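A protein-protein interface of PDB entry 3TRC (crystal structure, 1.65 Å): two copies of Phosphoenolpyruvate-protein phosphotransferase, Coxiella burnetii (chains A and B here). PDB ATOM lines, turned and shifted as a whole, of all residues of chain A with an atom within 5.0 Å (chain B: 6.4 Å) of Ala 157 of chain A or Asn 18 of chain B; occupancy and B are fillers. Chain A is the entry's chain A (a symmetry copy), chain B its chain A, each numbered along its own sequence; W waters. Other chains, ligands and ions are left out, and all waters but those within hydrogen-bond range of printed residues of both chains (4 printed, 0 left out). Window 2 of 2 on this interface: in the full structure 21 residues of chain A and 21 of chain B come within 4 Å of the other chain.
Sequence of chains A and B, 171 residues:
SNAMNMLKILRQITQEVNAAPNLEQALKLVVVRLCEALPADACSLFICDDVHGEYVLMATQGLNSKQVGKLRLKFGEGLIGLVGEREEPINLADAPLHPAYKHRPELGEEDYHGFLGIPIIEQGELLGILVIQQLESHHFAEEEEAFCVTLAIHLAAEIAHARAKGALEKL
The side-chain amide nitrogen (ND2) of Asn 18 of chain B sits at hydrogen-bond distance from the backbone carbonyl oxygen (O) of Ile 153 of chain A, 3.4 Å away. The backbone carbonyl oxygen (O) of Ala 19 of chain B sits close to the side-chain amide oxygen (OE1) of Gln 123 of chain A (3.2 Å).
The side-chain amide oxygen (OD1) of Asn 18 of chain B sits close to a ring nitrogen (NE2) of His 154 of chain B (3.1 Å).
CG2 of Thr 14 of chain B touches CG2 of Ile 153 of chain A (3.7 Å). N of Gln 15 of chain B touches CD1 of Ile 153 of chain A (3.9 Å). ND2 of Asn 18 of chain B touches CB of Ala 157 of chain A (3.5 Å).
Printed residues of chain B within 4 Å of Ile 153 of chain A: Thr 14, Gln 15 and Asn 18. Ala 157 of chain A touches just one residue of chain B: Asn 18 (3.5 Å). Ile 13 of chain B touches none of the printed residues of chain A. Of the printed residues of chain A, Thr 14 of chain B touches Ile 153. Printed residues of chain A within 4 Å of Ala 19 of chain B: Gln 123 (3.2 Å). Ala 20 of chain B touches none of the printed residues of chain A. The nearest residue of chain B that does not touch Ala 157 of chain A is His 154 of chain B (5.9 Å). The nearest printed residue of chain A that does not touch Ala 19 of chain B is Glu 122 of chain A (5.9 Å).
Along chain B the printed residues that touch a printed residue of chain A span positions 14 to 19. Among the printed residues, no Asp or Glu carboxylate lies within 4 Å of a Lys or Arg side-chain nitrogen of the other chain.
2 positions are printed for both chains. Of the 5 pairs that touch across the chains among the printed residues, none has its exchanged pair printed and touching as well.
Water W2 bridges a ring nitrogen (ND1) of His 154 of chain A (2.7 Å) and the side-chain amide nitrogen (ND2) of Asn 18 of chain B (3.3 Å). Water W1 bridges the side-chain carboxylate (OE2) of Glu 122 of chain A (2.8 Å) and the backbone carbonyl oxygen (O) of Asn 18 of chain B (3.4 Å). Water W4 lies within hydrogen-bond range of the side-chain carboxylate of Glu 122 of chain A (2.9 Å), the backbone carbonyl oxygen of Ile 153 of chain A (3.1 Å) and the side-chain amide nitrogen of Asn 18 of chain B (3.1 Å). Water W3 bridges the side-chain amide oxygen (OE1) of Gln 15 of chain B (3.1 Å) and the backbone NH (N) of Gln 123 of chain A (3.3 Å).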
ATOM      1  N   GLU A 122      22.308 -14.908 -22.821  1.00  0.00           N
ATOM      2  CA  GLU A 122      23.291 -15.745 -22.154  1.00  0.00           C
ATOM      3  C   GLU A 122      24.110 -16.454 -23.213  1.00  0.00           C
ATOM      4  O   GLU A 122      23.601 -17.320 -23.921  1.00  0.00           O
ATOM      5  CB  GLU A 122      22.601 -16.764 -21.251  1.00  0.00           C
ATOM      6  CG  GLU A 122      23.528 -17.834 -20.698  1.00  0.00           C
ATOM      7  CD  GLU A 122      24.476 -17.303 -19.641  1.00  0.00           C
ATOM      8  OE1 GLU A 122      24.313 -16.138 -19.218  1.00  0.00           O
ATOM      9  OE2 GLU A 122      25.385 -18.057 -19.234  1.00  0.00           O
ATOM     10  N   GLN A 123      25.378 -16.070 -23.324  1.00  0.00           N
ATOM     11  CA  GLN A 123      26.283 -16.663 -24.304  1.00  0.00           C
ATOM     12  C   GLN A 123      25.645 -16.825 -25.683  1.00  0.00           C
ATOM     13  O   GLN A 123      25.684 -17.906 -26.266  1.00  0.00           O
ATOM     14  CB  GLN A 123      26.796 -18.013 -23.806  1.00  0.00           C
ATOM     15  CG  GLN A 123      27.707 -17.914 -22.600  1.00  0.00           C
ATOM     16  CD  GLN A 123      28.379 -19.232 -22.276  1.00  0.00           C
ATOM     17  OE1 GLN A 123      29.569 -19.276 -21.973  1.00  0.00           O
ATOM     18  NE2 GLN A 123      27.616 -20.318 -22.341  1.00  0.00           N
ATOM     19  N   ILE A 153      23.284  -8.638 -18.122  1.00  0.00           N
ATOM     20  CA  ILE A 153      24.220  -9.756 -18.160  1.00  0.00           C
ATOM     21  C   ILE A 153      24.042 -10.610 -16.910  1.00  0.00           C
ATOM     22  O   ILE A 153      24.051 -11.839 -16.972  1.00  0.00           O
ATOM     23  CB  ILE A 153      25.671  -9.263 -18.266  1.00  0.00           C
ATOM     24  CG1 ILE A 153      25.834  -8.451 -19.554  1.00  0.00           C
ATOM     25  CG2 ILE A 153      26.642 -10.434 -18.232  1.00  0.00           C
ATOM     26  CD1 ILE A 153      27.146  -7.723 -19.673  1.00  0.00           C
ATOM     27  N   HIS A 154      23.863  -9.943 -15.776  1.00  0.00           N
ATOM     28  CA  HIS A 154      23.649 -10.621 -14.504  1.00  0.00           C
ATOM     29  C   HIS A 154      22.321 -11.374 -14.551  1.00  0.00           C
ATOM     30  O   HIS A 154      22.238 -12.536 -14.162  1.00  0.00           O
ATOM     31  CB  HIS A 154      23.646  -9.583 -13.376  1.00  0.00           C
ATOM     32  CG  HIS A 154      23.907 -10.144 -12.013  1.00  0.00           C
ATOM     33  ND1 HIS A 154      24.043 -11.496 -11.767  1.00  0.00           N
ATOM     34  CD2 HIS A 154      24.056  -9.531 -10.817  1.00  0.00           C
ATOM     35  CE1 HIS A 154      24.263 -11.687 -10.480  1.00  0.00           C
ATOM     36  NE2 HIS A 154      24.274 -10.509  -9.878  1.00  0.00           N
ATOM     37  N   LEU A 155      21.276 -10.702 -15.027  1.00  0.00           N
ATOM     38  CA  LEU A 155      19.959 -11.321 -15.142  1.00  0.00           C
ATOM     39  C   LEU A 155      19.984 -12.555 -16.039  1.00  0.00           C
ATOM     40  O   LEU A 155      19.325 -13.553 -15.748  1.00  0.00           O
ATOM     41  CB  LEU A 155      18.938 -10.310 -15.661  1.00  0.00           C
ATOM     42  CG  LEU A 155      18.775  -9.071 -14.774  1.00  0.00           C
ATOM     43  CD1 LEU A 155      17.772  -8.111 -15.383  1.00  0.00           C
ATOM     44  CD2 LEU A 155      18.349  -9.474 -13.372  1.00  0.00           C
ATOM     45  N   ALA A 156      20.743 -12.486 -17.128  1.00  0.00           N
ATOM     46  CA  ALA A 156      20.873 -13.630 -18.030  1.00  0.00           C
ATOM     47  C   ALA A 156      21.443 -14.837 -17.294  1.00  0.00           C
ATOM     48  O   ALA A 156      20.955 -15.963 -17.440  1.00  0.00           O
ATOM     49  CB  ALA A 156      21.745 -13.272 -19.233  1.00  0.00           C
ATOM     50  N   ALA A 157      22.480 -14.603 -16.495  1.00  0.00           N
ATOM     51  CA  ALA A 157      23.105 -15.681 -15.740  1.00  0.00           C
ATOM     52  C   ALA A 157      22.131 -16.270 -14.731  1.00  0.00           C
ATOM     53  O   ALA A 157      22.069 -17.482 -14.551  1.00  0.00           O
ATOM     54  CB  ALA A 157      24.363 -15.184 -15.033  1.00  0.00           C
ATOM     55  N   GLU A 158      21.372 -15.407 -14.070  1.00  0.00           N
ATOM     56  CA  GLU A 158      20.401 -15.859 -13.082  1.00  0.00           C
ATOM     57  C   GLU A 158      19.288 -16.697 -13.717  1.00  0.00           C
ATOM     58  O   GLU A 158      18.894 -17.730 -13.182  1.00  0.00           O
ATOM     59  CB  GLU A 158      19.836 -14.666 -12.309  1.00  0.00           C
ATOM     60  CG  GLU A 158      20.910 -13.887 -11.541  1.00  0.00           C
ATOM     61  CD  GLU A 158      21.541 -14.705 -10.422  1.00  0.00           C
ATOM     62  OE1 GLU A 158      20.785 -15.302  -9.634  1.00  0.00           O
ATOM     63  OE2 GLU A 158      22.788 -14.763 -10.336  1.00  0.00           O
ATOM     64  N   ILE A 159      18.788 -16.257 -14.866  1.00  0.00           N
ATOM     65  CA  ILE A 159      17.789 -17.026 -15.590  1.00  0.00           C
ATOM     66  C   ILE A 159      18.347 -18.364 -16.089  1.00  0.00           C
ATOM     67  O   ILE A 159      17.702 -19.407 -15.967  1.00  0.00           O
ATOM     68  CB  ILE A 159      17.215 -16.212 -16.763  1.00  0.00           C
ATOM     69  CG1 ILE A 159      16.539 -14.947 -16.219  1.00  0.00           C
ATOM     70  CG2 ILE A 159      16.257 -17.061 -17.595  1.00  0.00           C
ATOM     71  CD1 ILE A 159      16.053 -13.976 -17.292  1.00  0.00           C
ATOM     72  N   ALA A 160      19.551 -18.333 -16.645  1.00  0.00           N
ATOM     73  CA  ALA A 160      20.180 -19.558 -17.124  1.00  0.00           C
ATOM     74  C   ALA A 160      20.381 -20.557 -15.988  1.00  0.00           C
ATOM     75  O   ALA A 160      20.191 -21.764 -16.163  1.00  0.00           O
ATOM     76  CB  ALA A 160      21.500 -19.248 -17.810  1.00  0.00           C
ATOM     77  N   HIS A 161      20.768 -20.053 -14.820  1.00  0.00           N
ATOM     78  CA  HIS A 161      21.017 -20.915 -13.673  1.00  0.00           C
ATOM     79  C   HIS A 161      19.717 -21.556 -13.196  1.00  0.00           C
ATOM     80  O   HIS A 161      19.677 -22.749 -12.902  1.00  0.00           O
ATOM     81  CB  HIS A 161      21.680 -20.128 -12.539  1.00  0.00           C
ATOM     82  CG  HIS A 161      21.986 -20.951 -11.328  1.00  0.00           C
ATOM     83  ND1 HIS A 161      21.338 -20.775 -10.124  1.00  0.00           N
ATOM     84  CD2 HIS A 161      22.865 -21.963 -11.137  1.00  0.00           C
ATOM     85  CE1 HIS A 161      21.809 -21.639  -9.241  1.00  0.00           C
ATOM     86  NE2 HIS A 161      22.737 -22.371  -9.831  1.00  0.00           N
ATOM     87  N   ALA A 162      18.655 -20.756 -13.131  1.00  0.00           N
ATOM     88  CA  ALA A 162      17.338 -21.263 -12.751  1.00  0.00           C
ATOM     89  C   ALA A 162      16.869 -22.361 -13.702  1.00  0.00           C
ATOM     90  O   ALA A 162      16.352 -23.391 -13.268  1.00  0.00           O
ATOM     91  CB  ALA A 162      16.325 -20.130 -12.713  1.00  0.00           C
ATOM     92  N   ILE B  13      33.691  -6.914 -18.630  1.00  0.00           N
ATOM     93  CA  ILE B  13      34.228  -7.980 -17.789  1.00  0.00           C
ATOM     94  C   ILE B  13      33.135  -8.873 -17.201  1.00  0.00           C
ATOM     95  O   ILE B  13      33.338 -10.071 -17.032  1.00  0.00           O
ATOM     96  CB  ILE B  13      35.130  -7.439 -16.662  1.00  0.00           C
ATOM     97  CG1 ILE B  13      35.856  -8.587 -15.967  1.00  0.00           C
ATOM     98  CG2 ILE B  13      34.316  -6.646 -15.647  1.00  0.00           C
ATOM     99  CD1 ILE B  13      36.951  -8.127 -15.033  1.00  0.00           C
ATOM    100  N   THR B  14      31.983  -8.290 -16.885  1.00  0.00           N
ATOM    101  CA  THR B  14      30.858  -9.064 -16.365  1.00  0.00           C
ATOM    102  C   THR B  14      30.473 -10.068 -17.447  1.00  0.00           C
ATOM    103  O   THR B  14      30.198 -11.235 -17.168  1.00  0.00           O
ATOM    104  CB  THR B  14      29.655  -8.164 -16.006  1.00  0.00           C
ATOM    105  OG1 THR B  14      30.070  -7.168 -15.058  1.00  0.00           O
ATOM    106  CG2 THR B  14      28.528  -8.984 -15.393  1.00  0.00           C
ATOM    107  N   GLN B  15      30.482  -9.588 -18.688  1.00  0.00           N
ATOM    108  CA  GLN B  15      30.256 -10.413 -19.869  1.00  0.00           C
ATOM    109  C   GLN B  15      31.259 -11.558 -19.953  1.00  0.00           C
ATOM    110  O   GLN B  15      30.884 -12.720 -20.100  1.00  0.00           O
ATOM    111  CB  GLN B  15      30.385  -9.553 -21.126  1.00  0.00           C
ATOM    112  CG  GLN B  15      30.104 -10.286 -22.415  1.00  0.00           C
ATOM    113  CD  GLN B  15      28.634 -10.273 -22.764  1.00  0.00           C
ATOM    114  OE1 GLN B  15      27.856 -11.078 -22.252  1.00  0.00           O
ATOM    115  NE2 GLN B  15      28.240  -9.346 -23.630  1.00  0.00           N
ATOM    116  N   GLU B  16      32.540 -11.219 -19.867  1.00  0.00           N
ATOM    117  CA  GLU B  16      33.599 -12.212 -19.988  1.00  0.00           C
ATOM    118  C   GLU B  16      33.596 -13.239 -18.849  1.00  0.00           C
ATOM    119  O   GLU B  16      33.847 -14.420 -19.077  1.00  0.00           O
ATOM    120  CB  GLU B  16      34.970 -11.533 -20.105  1.00  0.00           C
ATOM    121  CG  GLU B  16      35.250 -10.910 -21.471  1.00  0.00           C
ATOM    122  CD  GLU B  16      36.658 -10.342 -21.577  1.00  0.00           C
ATOM    123  OE1 GLU B  16      37.214  -9.913 -20.544  1.00  0.00           O
ATOM    124  OE2 GLU B  16      37.215 -10.328 -22.694  1.00  0.00           O
ATOM    125  N   VAL B  17      33.309 -12.792 -17.629  1.00  0.00           N
ATOM    126  CA  VAL B  17      33.240 -13.706 -16.490  1.00  0.00           C
ATOM    127  C   VAL B  17      32.114 -14.719 -16.662  1.00  0.00           C
ATOM    128  O   VAL B  17      32.308 -15.914 -16.459  1.00  0.00           O
ATOM    129  CB  VAL B  17      33.066 -12.963 -15.147  1.00  0.00           C
ATOM    130  CG1 VAL B  17      32.780 -13.957 -14.019  1.00  0.00           C
ATOM    131  CG2 VAL B  17      34.303 -12.136 -14.832  1.00  0.00           C
ATOM    132  N   ASN B  18      30.935 -14.244 -17.048  1.00  0.00           N
ATOM    133  CA  ASN B  18      29.811 -15.156 -17.220  1.00  0.00           C
ATOM    134  C   ASN B  18      29.994 -16.116 -18.393  1.00  0.00           C
ATOM    135  O   ASN B  18      29.391 -17.183 -18.422  1.00  0.00           O
ATOM    136  CB  ASN B  18      28.489 -14.391 -17.318  1.00  0.00           C
ATOM    137  CG  ASN B  18      27.977 -13.953 -15.962  1.00  0.00           C
ATOM    138  OD1 ASN B  18      28.446 -14.432 -14.928  1.00  0.00           O
ATOM    139  ND2 ASN B  18      27.006 -13.049 -15.956  1.00  0.00           N
ATOM    140  N   ALA B  19      30.844 -15.742 -19.346  1.00  0.00           N
ATOM    141  CA  ALA B  19      31.125 -16.585 -20.510  1.00  0.00           C
ATOM    142  C   ALA B  19      32.292 -17.547 -20.279  1.00  0.00           C
ATOM    143  O   ALA B  19      32.523 -18.459 -21.070  1.00  0.00           O
ATOM    144  CB  ALA B  19      31.383 -15.726 -21.742  1.00  0.00           C
ATOM    145  N   ALA B  20      33.030 -17.337 -19.196  1.00  0.00           N
ATOM    146  CA  ALA B  20      34.142 -18.217 -18.862  1.00  0.00           C
ATOM    147  C   ALA B  20      33.652 -19.643 -18.634  1.00  0.00           C
ATOM    148  O   ALA B  20      32.619 -19.861 -18.007  1.00  0.00           O
ATOM    149  CB  ALA B  20      34.874 -17.702 -17.633  1.00  0.00           C
ATOM    150  N   PRO B  21      34.405 -20.626 -19.138  1.00  0.00           N
ATOM    151  CA  PRO B  21      34.005 -22.036 -19.061  1.00  0.00           C
ATOM    152  C   PRO B  21      34.209 -22.685 -17.686  1.00  0.00           C
ATOM    153  O   PRO B  21      33.632 -23.741 -17.424  1.00  0.00           O
ATOM    154  CB  PRO B  21      34.892 -22.704 -20.115  1.00  0.00           C
ATOM    155  CG  PRO B  21      36.088 -21.822 -20.221  1.00  0.00           C
ATOM    156  CD  PRO B  21      35.632 -20.427 -19.931  1.00  0.00           C
ATOM    157  N   ALA B  26      37.775 -17.747 -15.104  1.00  0.00           N
ATOM    158  CA  ALA B  26      37.165 -16.484 -14.696  1.00  0.00           C
ATOM    159  C   ALA B  26      38.125 -15.674 -13.837  1.00  0.00           C
ATOM    160  O   ALA B  26      38.275 -14.468 -14.025  1.00  0.00           O
ATOM    161  CB  ALA B  26      35.863 -16.725 -13.952  1.00  0.00           C
ATOM    162  N   HIS B 154      30.496 -10.342  -7.767  1.00  0.00           N
ATOM    163  CA  HIS B 154      30.381 -11.311  -8.849  1.00  0.00           C
ATOM    164  C   HIS B 154      31.326 -12.482  -8.580  1.00  0.00           C
ATOM    165  O   HIS B 154      30.945 -13.642  -8.701  1.00  0.00           O
ATOM    166  CB  HIS B 154      30.728 -10.627 -10.176  1.00  0.00           C
ATOM    167  CG  HIS B 154      30.215 -11.331 -11.392  1.00  0.00           C
ATOM    168  ND1 HIS B 154      29.566 -12.549 -11.342  1.00  0.00           N
ATOM    169  CD2 HIS B 154      30.257 -10.986 -12.700  1.00  0.00           C
ATOM    170  CE1 HIS B 154      29.233 -12.920 -12.564  1.00  0.00           C
ATOM    171  NE2 HIS B 154      29.644 -11.989 -13.410  1.00  0.00           N
ATOM    172  N   GLU B 158      30.654 -16.572  -8.123  1.00  0.00           N
ATOM    173  CA  GLU B 158      31.337 -17.563  -8.944  1.00  0.00           C
ATOM    174  C   GLU B 158      32.075 -18.598  -8.092  1.00  0.00           C
ATOM    175  O   GLU B 158      32.025 -19.795  -8.369  1.00  0.00           O
ATOM    176  CB  GLU B 158      32.277 -16.874  -9.934  1.00  0.00           C
ATOM    177  CG  GLU B 158      31.546 -15.936 -10.901  1.00  0.00           C
ATOM    178  CD  GLU B 158      30.603 -16.677 -11.839  1.00  0.00           C
ATOM    179  OE1 GLU B 158      31.042 -17.673 -12.443  1.00  0.00           O
ATOM    180  OE2 GLU B 158      29.425 -16.276 -11.965  1.00  0.00           O
HETATM  181  O   HOH W   1      26.529 -17.666 -16.722  1.00  0.00           O
HETATM  182  O   HOH W   2      25.926 -13.038 -12.840  1.00  0.00           O
HETATM  183  O   HOH W   3      26.349 -13.602 -21.306  1.00  0.00           O
HETATM  184  O   HOH W   4      25.790 -13.706 -18.749  1.00  0.00           O
